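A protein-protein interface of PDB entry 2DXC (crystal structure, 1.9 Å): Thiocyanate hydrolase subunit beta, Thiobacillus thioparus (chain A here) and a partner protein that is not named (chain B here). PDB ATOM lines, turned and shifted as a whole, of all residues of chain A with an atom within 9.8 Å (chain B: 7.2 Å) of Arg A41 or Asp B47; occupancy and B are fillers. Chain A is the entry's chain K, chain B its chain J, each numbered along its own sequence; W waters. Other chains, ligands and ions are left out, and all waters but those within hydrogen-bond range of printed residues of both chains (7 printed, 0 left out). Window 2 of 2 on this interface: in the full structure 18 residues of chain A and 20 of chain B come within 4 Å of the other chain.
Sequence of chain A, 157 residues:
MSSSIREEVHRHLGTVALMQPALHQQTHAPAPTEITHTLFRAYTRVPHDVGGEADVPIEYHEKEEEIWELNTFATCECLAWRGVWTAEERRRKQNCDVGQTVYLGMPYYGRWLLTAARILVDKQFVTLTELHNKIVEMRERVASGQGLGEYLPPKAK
The guanidinium group of Arg B61 sits at hydrogen-bond distance from the backbone carbonyl oxygen of Met B57 (3.4 Å). The guanidinium group (NH2) of Arg A45 lies within hydrogen-bond range of the backbone carbonyl oxygen (O) of Asp A49 (2.7 Å). The side-chain carboxylate of Asp B47 is in salt-bridge range of the guanidinium group of Arg B61, at 3.1 Å.
The side-chain carboxylate of Asp A49 is in hydrogen-bond range of the side-chain hydroxyl of Thr B58. The side-chain carboxylate (OD2) of Asp B47 lies within salt-bridge range of the guanidinium group (NH1) of Arg A41 (3.0 Å).
Of chain B, only Asp B47 and Thr B58 come within 4 Å of Arg A41. Of chain A, only Arg A41 (3.0 Å) comes within 4 Å of Asp B47. Leu B48 touches none of the printed residues of chain A. Of the printed residues of chain A, Thr B58 touches Arg A41 (3.9 Å) and Asp A49 (2.6 Å). Of the printed residues of chain B, Val A46 touches Asp B50. The nearest residue of chain B that does not touch Arg A41 is Arg B61 (4.2 Å).
Thr B58 touches Arg A41. Val A46 touches Asp B50 (CG2 to O, 3.4 Å). Asp A49 touches Met B57.
Hydrophobic or aromatic side chains of chain B that line the printed part of chain A: Met B57. Among the printed residues, 5 pairs touch across the chains. Among the printed residues, Asp or Glu carboxylates within 4 Å of a Lys or Arg side-chain nitrogen of the other chain: Arg A41 with Asp B47 (3.0 Å).
Water W3 lies within hydrogen-bond range of the backbone carbonyl oxygen of Leu B48 (2.7 Å), the side-chain carboxylate of Asp B47 (2.8 Å) and the guanidinium group of Arg A41 (3.4 Å). Water W1 lies within hydrogen-bond range of OD1 of Asp A49 (2.7 Å), N of Tyr B59 (3.1 Å) and N of Thr B58 (3.4 Å). Water W4 lies within hydrogen-bond range of OD1 of Asp B50 (2.8 Å) and NE of Arg A41 (3.2 Å). Water W6 lies within hydrogen-bond range of the side-chain carboxylate of Asp B50 (2.8 Å), the side-chain hydroxyl of Thr B58 (2.9 Å), the guanidinium group of Arg A41 (3.2 Å) and the guanidinium group of Arg B61 (3.3 Å). Water W5 lies within hydrogen-bond range of the side-chain hydroxyl (OG1) of Thr A44 (2.8 Å) and the side-chain carboxylate (OD1) of Asp B50 (3.0 Å). Water W2 bridges the backbone NH of Val A46 (2.8 Å) and the side-chain carboxylate of Asp B50 (3.2 Å).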
ATOM      1  N   ILE A  35       4.015 -33.477 -16.700  1.00  0.00           N
ATOM      2  CA  ILE A  35       4.791 -32.769 -15.694  1.00  0.00           C
ATOM      3  C   ILE A  35       5.889 -31.950 -16.350  1.00  0.00           C
ATOM      4  O   ILE A  35       6.808 -32.504 -16.947  1.00  0.00           O
ATOM      5  CB  ILE A  35       5.441 -33.751 -14.698  1.00  0.00           C
ATOM      6  CG1 ILE A  35       4.362 -34.622 -14.057  1.00  0.00           C
ATOM      7  CG2 ILE A  35       6.193 -32.982 -13.618  1.00  0.00           C
ATOM      8  CD1 ILE A  35       3.332 -33.845 -13.214  1.00  0.00           C
ATOM      9  N   THR A  36       5.783 -30.631 -16.240  1.00  0.00           N
ATOM     10  CA  THR A  36       6.784 -29.731 -16.794  1.00  0.00           C
ATOM     11  C   THR A  36       7.838 -29.542 -15.710  1.00  0.00           C
ATOM     12  O   THR A  36       7.621 -29.933 -14.563  1.00  0.00           O
ATOM     13  CB  THR A  36       6.184 -28.355 -17.102  1.00  0.00           C
ATOM     14  OG1 THR A  36       5.623 -27.811 -15.903  1.00  0.00           O
ATOM     15  CG2 THR A  36       5.094 -28.467 -18.163  1.00  0.00           C
ATOM     16  N   HIS A  37       8.975 -28.948 -16.061  1.00  0.00           N
ATOM     17  CA  HIS A  37      10.009 -28.721 -15.061  1.00  0.00           C
ATOM     18  C   HIS A  37       9.437 -27.814 -13.982  1.00  0.00           C
ATOM     19  O   HIS A  37       9.737 -27.971 -12.800  1.00  0.00           O
ATOM     20  CB  HIS A  37      11.248 -28.053 -15.664  1.00  0.00           C
ATOM     21  CG  HIS A  37      12.197 -27.534 -14.631  1.00  0.00           C
ATOM     22  ND1 HIS A  37      12.856 -28.360 -13.744  1.00  0.00           N
ATOM     23  CD2 HIS A  37      12.533 -26.268 -14.284  1.00  0.00           C
ATOM     24  CE1 HIS A  37      13.552 -27.626 -12.894  1.00  0.00           C
ATOM     25  NE2 HIS A  37      13.372 -26.353 -13.199  1.00  0.00           N
ATOM     26  N   THR A  38       8.613 -26.861 -14.401  1.00  0.00           N
ATOM     27  CA  THR A  38       7.994 -25.928 -13.470  1.00  0.00           C
ATOM     28  C   THR A  38       7.163 -26.678 -12.428  1.00  0.00           C
ATOM     29  O   THR A  38       7.271 -26.416 -11.232  1.00  0.00           O
ATOM     30  CB  THR A  38       7.100 -24.915 -14.215  1.00  0.00           C
ATOM     31  OG1 THR A  38       7.912 -24.115 -15.083  1.00  0.00           O
ATOM     32  CG2 THR A  38       6.374 -24.006 -13.225  1.00  0.00           C
ATOM     33  N   LEU A  39       6.335 -27.612 -12.886  1.00  0.00           N
ATOM     34  CA  LEU A  39       5.515 -28.396 -11.970  1.00  0.00           C
ATOM     35  C   LEU A  39       6.384 -29.327 -11.126  1.00  0.00           C
ATOM     36  O   LEU A  39       6.135 -29.511  -9.936  1.00  0.00           O
ATOM     37  CB  LEU A  39       4.480 -29.215 -12.746  1.00  0.00           C
ATOM     38  CG  LEU A  39       3.299 -28.441 -13.340  1.00  0.00           C
ATOM     39  CD1 LEU A  39       2.391 -29.399 -14.096  1.00  0.00           C
ATOM     40  CD2 LEU A  39       2.525 -27.748 -12.224  1.00  0.00           C
ATOM     41  N   PHE A  40       7.405 -29.918 -11.744  1.00  0.00           N
ATOM     42  CA  PHE A  40       8.297 -30.817 -11.022  1.00  0.00           C
ATOM     43  C   PHE A  40       8.904 -30.083  -9.822  1.00  0.00           C
ATOM     44  O   PHE A  40       8.913 -30.600  -8.704  1.00  0.00           O
ATOM     45  CB  PHE A  40       9.429 -31.309 -11.932  1.00  0.00           C
ATOM     46  CG  PHE A  40      10.334 -32.323 -11.280  1.00  0.00           C
ATOM     47  CD1 PHE A  40      10.066 -33.686 -11.380  1.00  0.00           C
ATOM     48  CD2 PHE A  40      11.442 -31.912 -10.541  1.00  0.00           C
ATOM     49  CE1 PHE A  40      10.889 -34.627 -10.752  1.00  0.00           C
ATOM     50  CE2 PHE A  40      12.269 -32.843  -9.909  1.00  0.00           C
ATOM     51  CZ  PHE A  40      11.992 -34.204 -10.015  1.00  0.00           C
ATOM     52  N   ARG A  41       9.408 -28.876 -10.056  1.00  0.00           N
ATOM     53  CA  ARG A  41      10.017 -28.109  -8.972  1.00  0.00           C
ATOM     54  C   ARG A  41       8.997 -27.729  -7.902  1.00  0.00           C
ATOM     55  O   ARG A  41       9.303 -27.751  -6.708  1.00  0.00           O
ATOM     56  CB  ARG A  41      10.696 -26.846  -9.513  1.00  0.00           C
ATOM     57  CG  ARG A  41      11.363 -26.014  -8.419  1.00  0.00           C
ATOM     58  CD  ARG A  41      12.247 -24.904  -8.974  1.00  0.00           C
ATOM     59  NE  ARG A  41      12.953 -24.218  -7.894  1.00  0.00           N
ATOM     60  CZ  ARG A  41      14.109 -23.575  -8.038  1.00  0.00           C
ATOM     61  NH1 ARG A  41      14.701 -23.521  -9.222  1.00  0.00           N
ATOM     62  NH2 ARG A  41      14.686 -23.007  -6.987  1.00  0.00           N
ATOM     63  N   ALA A  42       7.787 -27.387  -8.327  1.00  0.00           N
ATOM     64  CA  ALA A  42       6.731 -27.012  -7.393  1.00  0.00           C
ATOM     65  C   ALA A  42       6.268 -28.207  -6.547  1.00  0.00           C
ATOM     66  O   ALA A  42       5.980 -28.057  -5.361  1.00  0.00           O
ATOM     67  CB  ALA A  42       5.550 -26.418  -8.153  1.00  0.00           C
ATOM     68  N   TYR A  43       6.195 -29.389  -7.154  1.00  0.00           N
ATOM     69  CA  TYR A  43       5.770 -30.588  -6.432  1.00  0.00           C
ATOM     70  C   TYR A  43       6.837 -31.125  -5.480  1.00  0.00           C
ATOM     71  O   TYR A  43       6.516 -31.634  -4.402  1.00  0.00           O
ATOM     72  CB  TYR A  43       5.374 -31.700  -7.416  1.00  0.00           C
ATOM     73  CG  TYR A  43       3.956 -31.597  -7.947  1.00  0.00           C
ATOM     74  CD1 TYR A  43       2.862 -31.627  -7.077  1.00  0.00           C
ATOM     75  CD2 TYR A  43       3.710 -31.456  -9.315  1.00  0.00           C
ATOM     76  CE1 TYR A  43       1.552 -31.512  -7.556  1.00  0.00           C
ATOM     77  CE2 TYR A  43       2.403 -31.341  -9.805  1.00  0.00           C
ATOM     78  CZ  TYR A  43       1.330 -31.367  -8.918  1.00  0.00           C
ATOM     79  OH  TYR A  43       0.041 -31.229  -9.387  1.00  0.00           O
ATOM     80  N   THR A  44       8.102 -31.018  -5.874  1.00  0.00           N
ATOM     81  CA  THR A  44       9.190 -31.520  -5.043  1.00  0.00           C
ATOM     82  C   THR A  44       9.781 -30.452  -4.124  1.00  0.00           C
ATOM     83  O   THR A  44      10.808 -30.670  -3.481  1.00  0.00           O
ATOM     84  CB  THR A  44      10.317 -32.131  -5.908  1.00  0.00           C
ATOM     85  OG1 THR A  44      10.857 -31.133  -6.781  1.00  0.00           O
ATOM     86  CG2 THR A  44       9.774 -33.278  -6.746  1.00  0.00           C
ATOM     87  N   ARG A  45       9.115 -29.303  -4.068  1.00  0.00           N
ATOM     88  CA  ARG A  45       9.519 -28.178  -3.225  1.00  0.00           C
ATOM     89  C   ARG A  45       9.540 -28.645  -1.773  1.00  0.00           C
ATOM     90  O   ARG A  45       8.968 -29.682  -1.443  1.00  0.00           O
ATOM     91  CB  ARG A  45       8.472 -27.060  -3.305  1.00  0.00           C
ATOM     92  CG  ARG A  45       7.180 -27.475  -2.570  1.00  0.00           C
ATOM     93  CD  ARG A  45       6.138 -26.376  -2.424  1.00  0.00           C
ATOM     94  NE  ARG A  45       6.673 -25.200  -1.754  1.00  0.00           N
ATOM     95  CZ  ARG A  45       5.927 -24.221  -1.257  1.00  0.00           C
ATOM     96  NH1 ARG A  45       4.602 -24.274  -1.343  1.00  0.00           N
ATOM     97  NH2 ARG A  45       6.512 -23.172  -0.695  1.00  0.00           N
ATOM     98  N   VAL A  46      10.170 -27.857  -0.912  1.00  0.00           N
ATOM     99  CA  VAL A  46      10.201 -28.149   0.514  1.00  0.00           C
ATOM    100  C   VAL A  46       9.054 -27.276   1.039  1.00  0.00           C
ATOM    101  O   VAL A  46       9.133 -26.050   0.994  1.00  0.00           O
ATOM    102  CB  VAL A  46      11.537 -27.700   1.141  1.00  0.00           C
ATOM    103  CG1 VAL A  46      11.764 -28.431   2.431  1.00  0.00           C
ATOM    104  CG2 VAL A  46      12.685 -27.965   0.179  1.00  0.00           C
ATOM    105  N   PRO A  47       7.971 -27.897   1.533  1.00  0.00           N
ATOM    106  CA  PRO A  47       6.779 -27.222   2.062  1.00  0.00           C
ATOM    107  C   PRO A  47       6.963 -25.993   2.958  1.00  0.00           C
ATOM    108  O   PRO A  47       6.165 -25.057   2.890  1.00  0.00           O
ATOM    109  CB  PRO A  47       6.041 -28.344   2.795  1.00  0.00           C
ATOM    110  CG  PRO A  47       6.400 -29.550   2.001  1.00  0.00           C
ATOM    111  CD  PRO A  47       7.879 -29.352   1.751  1.00  0.00           C
ATOM    112  N   ASP A  49       9.216 -23.655   2.863  1.00  0.00           N
ATOM    113  CA  ASP A  49       9.795 -22.507   2.172  1.00  0.00           C
ATOM    114  C   ASP A  49       8.711 -21.640   1.520  1.00  0.00           C
ATOM    115  O   ASP A  49       8.527 -21.678   0.305  1.00  0.00           O
ATOM    116  CB  ASP A  49      10.784 -23.028   1.122  1.00  0.00           C
ATOM    117  CG  ASP A  49      11.629 -21.934   0.516  1.00  0.00           C
ATOM    118  OD1 ASP A  49      11.586 -20.793   1.025  1.00  0.00           O
ATOM    119  OD2 ASP A  49      12.343 -22.222  -0.469  1.00  0.00           O
ATOM    120  N   GLN A 100       2.823 -31.188   1.587  1.00  0.00           N
ATOM    121  CA  GLN A 100       2.007 -29.992   1.374  1.00  0.00           C
ATOM    122  C   GLN A 100       0.633 -29.946   2.059  1.00  0.00           C
ATOM    123  O   GLN A 100       0.314 -28.976   2.748  1.00  0.00           O
ATOM    124  CB  GLN A 100       1.827 -29.777  -0.136  1.00  0.00           C
ATOM    125  CG  GLN A 100       1.138 -28.483  -0.546  1.00  0.00           C
ATOM    126  CD  GLN A 100       1.924 -27.250  -0.143  1.00  0.00           C
ATOM    127  OE1 GLN A 100       1.875 -26.820   1.012  1.00  0.00           O
ATOM    128  NE2 GLN A 100       2.663 -26.684  -1.090  1.00  0.00           N
ATOM    129  N   ARG B  44      26.872 -14.294  -4.839  1.00  0.00           N
ATOM    130  CA  ARG B  44      25.638 -14.660  -5.517  1.00  0.00           C
ATOM    131  C   ARG B  44      25.213 -16.009  -4.950  1.00  0.00           C
ATOM    132  O   ARG B  44      26.058 -16.855  -4.663  1.00  0.00           O
ATOM    133  CB  ARG B  44      25.874 -14.779  -7.024  1.00  0.00           C
ATOM    134  CG  ARG B  44      24.617 -15.083  -7.832  1.00  0.00           C
ATOM    135  CD  ARG B  44      24.929 -15.341  -9.310  1.00  0.00           C
ATOM    136  NE  ARG B  44      25.585 -14.204  -9.956  1.00  0.00           N
ATOM    137  CZ  ARG B  44      26.904 -14.026 -10.031  1.00  0.00           C
ATOM    138  NH1 ARG B  44      27.736 -14.915  -9.504  1.00  0.00           N
ATOM    139  NH2 ARG B  44      27.394 -12.945 -10.631  1.00  0.00           N
ATOM    140  N   ILE B  45      23.909 -16.209  -4.790  1.00  0.00           N
ATOM    141  CA  ILE B  45      23.403 -17.459  -4.241  1.00  0.00           C
ATOM    142  C   ILE B  45      23.182 -18.505  -5.330  1.00  0.00           C
ATOM    143  O   ILE B  45      22.352 -18.319  -6.223  1.00  0.00           O
ATOM    144  CB  ILE B  45      22.071 -17.241  -3.496  1.00  0.00           C
ATOM    145  CG1 ILE B  45      22.207 -16.067  -2.523  1.00  0.00           C
ATOM    146  CG2 ILE B  45      21.683 -18.497  -2.737  1.00  0.00           C
ATOM    147  CD1 ILE B  45      23.336 -16.213  -1.483  1.00  0.00           C
ATOM    148  N   LYS B  46      23.920 -19.606  -5.241  1.00  0.00           N
ATOM    149  CA  LYS B  46      23.807 -20.693  -6.207  1.00  0.00           C
ATOM    150  C   LYS B  46      22.474 -21.410  -6.017  1.00  0.00           C
ATOM    151  O   LYS B  46      22.047 -21.653  -4.888  1.00  0.00           O
ATOM    152  CB  LYS B  46      24.963 -21.683  -6.017  1.00  0.00           C
ATOM    153  CG  LYS B  46      26.342 -21.045  -6.142  1.00  0.00           C
ATOM    154  CD  LYS B  46      27.472 -21.995  -5.757  1.00  0.00           C
ATOM    155  CE  LYS B  46      27.621 -23.136  -6.746  1.00  0.00           C
ATOM    156  NZ  LYS B  46      28.811 -23.987  -6.432  1.00  0.00           N
ATOM    157  N   ASP B  47      21.820 -21.751  -7.120  1.00  0.00           N
ATOM    158  CA  ASP B  47      20.536 -22.443  -7.050  1.00  0.00           C
ATOM    159  C   ASP B  47      20.765 -23.949  -7.025  1.00  0.00           C
ATOM    160  O   ASP B  47      20.476 -24.655  -7.991  1.00  0.00           O
ATOM    161  CB  ASP B  47      19.652 -22.046  -8.241  1.00  0.00           C
ATOM    162  CG  ASP B  47      18.231 -22.576  -8.118  1.00  0.00           C
ATOM    163  OD1 ASP B  47      17.781 -22.814  -6.976  1.00  0.00           O
ATOM    164  OD2 ASP B  47      17.556 -22.738  -9.159  1.00  0.00           O
ATOM    165  N   LEU B  48      21.296 -24.432  -5.904  1.00  0.00           N
ATOM    166  CA  LEU B  48      21.575 -25.852  -5.728  1.00  0.00           C
ATOM    167  C   LEU B  48      20.271 -26.626  -5.615  1.00  0.00           C
ATOM    168  O   LEU B  48      19.260 -26.086  -5.166  1.00  0.00           O
ATOM    169  CB  LEU B  48      22.404 -26.068  -4.457  1.00  0.00           C
ATOM    170  CG  LEU B  48      23.744 -25.331  -4.391  1.00  0.00           C
ATOM    171  CD1 LEU B  48      24.477 -25.689  -3.102  1.00  0.00           C
ATOM    172  CD2 LEU B  48      24.586 -25.716  -5.598  1.00  0.00           C
ATOM    173  N   PRO B  49      20.273 -27.906  -6.029  1.00  0.00           N
ATOM    174  CA  PRO B  49      19.051 -28.712  -5.943  1.00  0.00           C
ATOM    175  C   PRO B  49      18.538 -28.664  -4.510  1.00  0.00           C
ATOM    176  O   PRO B  49      19.332 -28.646  -3.567  1.00  0.00           O
ATOM    177  CB  PRO B  49      19.530 -30.108  -6.337  1.00  0.00           C
ATOM    178  CG  PRO B  49      20.648 -29.817  -7.296  1.00  0.00           C
ATOM    179  CD  PRO B  49      21.382 -28.690  -6.599  1.00  0.00           C
ATOM    180  N   ASP B  50      17.220 -28.642  -4.343  1.00  0.00           N
ATOM    181  CA  ASP B  50      16.629 -28.573  -3.012  1.00  0.00           C
ATOM    182  C   ASP B  50      15.751 -29.773  -2.672  1.00  0.00           C
ATOM    183  O   ASP B  50      14.940 -29.717  -1.752  1.00  0.00           O
ATOM    184  CB  ASP B  50      15.817 -27.283  -2.872  1.00  0.00           C
ATOM    185  CG  ASP B  50      14.686 -27.182  -3.886  1.00  0.00           C
ATOM    186  OD1 ASP B  50      14.540 -28.094  -4.731  1.00  0.00           O
ATOM    187  OD2 ASP B  50      13.936 -26.182  -3.837  1.00  0.00           O
ATOM    188  N   THR B  56      17.974 -22.760   2.622  1.00  0.00           N
ATOM    189  CA  THR B  56      18.368 -21.591   1.842  1.00  0.00           C
ATOM    190  C   THR B  56      17.129 -21.309   0.996  1.00  0.00           C
ATOM    191  O   THR B  56      16.918 -21.928  -0.051  1.00  0.00           O
ATOM    192  CB  THR B  56      19.572 -21.887   0.933  1.00  0.00           C
ATOM    193  OG1 THR B  56      20.703 -22.234   1.741  1.00  0.00           O
ATOM    194  CG2 THR B  56      19.913 -20.664   0.085  1.00  0.00           C
ATOM    195  N   MET B  57      16.305 -20.388   1.486  1.00  0.00           N
ATOM    196  CA  MET B  57      15.044 -20.031   0.846  1.00  0.00           C
ATOM    197  C   MET B  57      15.103 -19.856  -0.662  1.00  0.00           C
ATOM    198  O   MET B  57      16.074 -19.336  -1.208  1.00  0.00           O
ATOM    199  CB  MET B  57      14.468 -18.758   1.477  1.00  0.00           C
ATOM    200  CG  MET B  57      14.166 -18.852   2.974  1.00  0.00           C
ATOM    201  SD  MET B  57      15.642 -18.889   4.020  1.00  0.00           S
ATOM    202  CE  MET B  57      16.289 -17.239   3.744  1.00  0.00           C
ATOM    203  N   THR B  58      14.042 -20.293  -1.331  1.00  0.00           N
ATOM    204  CA  THR B  58      13.953 -20.172  -2.774  1.00  0.00           C
ATOM    205  C   THR B  58      14.043 -18.701  -3.188  1.00  0.00           C
ATOM    206  O   THR B  58      14.691 -18.378  -4.183  1.00  0.00           O
ATOM    207  CB  THR B  58      12.625 -20.762  -3.303  1.00  0.00           C
ATOM    208  OG1 THR B  58      12.579 -22.165  -3.018  1.00  0.00           O
ATOM    209  CG2 THR B  58      12.506 -20.556  -4.806  1.00  0.00           C
ATOM    210  N   TYR B  59      13.426 -17.810  -2.413  1.00  0.00           N
ATOM    211  CA  TYR B  59      13.436 -16.390  -2.759  1.00  0.00           C
ATOM    212  C   TYR B  59      14.818 -15.742  -2.858  1.00  0.00           C
ATOM    213  O   TYR B  59      14.945 -14.635  -3.390  1.00  0.00           O
ATOM    214  CB  TYR B  59      12.521 -15.585  -1.806  1.00  0.00           C
ATOM    215  CG  TYR B  59      13.040 -15.300  -0.403  1.00  0.00           C
ATOM    216  CD1 TYR B  59      14.030 -14.343  -0.179  1.00  0.00           C
ATOM    217  CD2 TYR B  59      12.494 -15.946   0.705  1.00  0.00           C
ATOM    218  CE1 TYR B  59      14.461 -14.034   1.124  1.00  0.00           C
ATOM    219  CE2 TYR B  59      12.914 -15.647   2.004  1.00  0.00           C
ATOM    220  CZ  TYR B  59      13.896 -14.692   2.207  1.00  0.00           C
ATOM    221  OH  TYR B  59      14.312 -14.398   3.487  1.00  0.00           O
ATOM    222  N   ARG B  61      17.575 -17.505  -4.238  1.00  0.00           N
ATOM    223  CA  ARG B  61      18.320 -18.125  -5.336  1.00  0.00           C
ATOM    224  C   ARG B  61      18.641 -17.194  -6.499  1.00  0.00           C
ATOM    225  O   ARG B  61      17.751 -16.571  -7.083  1.00  0.00           O
ATOM    226  CB  ARG B  61      17.581 -19.366  -5.867  1.00  0.00           C
ATOM    227  CG  ARG B  61      17.173 -20.398  -4.804  1.00  0.00           C
ATOM    228  CD  ARG B  61      18.293 -20.681  -3.805  1.00  0.00           C
ATOM    229  NE  ARG B  61      17.923 -21.701  -2.821  1.00  0.00           N
ATOM    230  CZ  ARG B  61      18.107 -23.009  -2.986  1.00  0.00           C
ATOM    231  NH1 ARG B  61      18.658 -23.470  -4.104  1.00  0.00           N
ATOM    232  NH2 ARG B  61      17.758 -23.856  -2.026  1.00  0.00           N
ATOM    233  N   GLY B  62      19.925 -17.106  -6.830  1.00  0.00           N
ATOM    234  CA  GLY B  62      20.344 -16.266  -7.934  1.00  0.00           C
ATOM    235  C   GLY B  62      20.514 -14.799  -7.591  1.00  0.00           C
ATOM    236  O   GLY B  62      20.959 -14.016  -8.428  1.00  0.00           O
ATOM    237  N   TYR B 122      26.525 -22.537  -0.768  1.00  0.00           N
ATOM    238  CA  TYR B 122      25.616 -21.812  -1.659  1.00  0.00           C
ATOM    239  C   TYR B 122      26.197 -20.528  -2.238  1.00  0.00           C
ATOM    240  O   TYR B 122      25.588 -19.902  -3.107  1.00  0.00           O
ATOM    241  CB  TYR B 122      24.329 -21.452  -0.909  1.00  0.00           C
ATOM    242  CG  TYR B 122      23.419 -22.621  -0.631  1.00  0.00           C
ATOM    243  CD1 TYR B 122      22.516 -23.071  -1.594  1.00  0.00           C
ATOM    244  CD2 TYR B 122      23.473 -23.293   0.589  1.00  0.00           C
ATOM    245  CE1 TYR B 122      21.687 -24.161  -1.348  1.00  0.00           C
ATOM    246  CE2 TYR B 122      22.653 -24.383   0.846  1.00  0.00           C
ATOM    247  CZ  TYR B 122      21.763 -24.810  -0.128  1.00  0.00           C
ATOM    248  OH  TYR B 122      20.951 -25.885   0.122  1.00  0.00           O
ATOM    249  N   GLU B 124      29.027 -17.981  -4.192  1.00  0.00           N
ATOM    250  CA  GLU B 124      30.027 -17.867  -5.244  1.00  0.00           C
ATOM    251  C   GLU B 124      30.300 -16.375  -5.394  1.00  0.00           C
ATOM    252  O   GLU B 124      29.385 -15.557  -5.277  1.00  0.00           O
ATOM    253  CB  GLU B 124      29.537 -18.459  -6.571  1.00  0.00           C
ATOM    254  CG  GLU B 124      28.272 -17.843  -7.132  1.00  0.00           C
ATOM    255  CD  GLU B 124      27.962 -18.339  -8.536  1.00  0.00           C
ATOM    256  OE1 GLU B 124      28.263 -19.513  -8.839  1.00  0.00           O
ATOM    257  OE2 GLU B 124      27.407 -17.557  -9.335  1.00  0.00           O
HETATM  258  O   HOH W   1      11.036 -18.832  -0.759  1.00  0.00           O
HETATM  259  O   HOH W   2      11.451 -25.516  -1.912  1.00  0.00           O
HETATM  260  O   HOH W   3      17.005 -25.490  -6.527  1.00  0.00           O
HETATM  261  O   HOH W   4      14.771 -26.786  -7.193  1.00  0.00           O
HETATM  262  O   HOH W   5      13.469 -30.063  -6.676  1.00  0.00           O
HETATM  263  O   HOH W   6      14.995 -23.587  -3.898  1.00  0.00           O
HETATM  264  O   HOH W   7      12.226 -24.170  -5.247  1.00  0.00           O
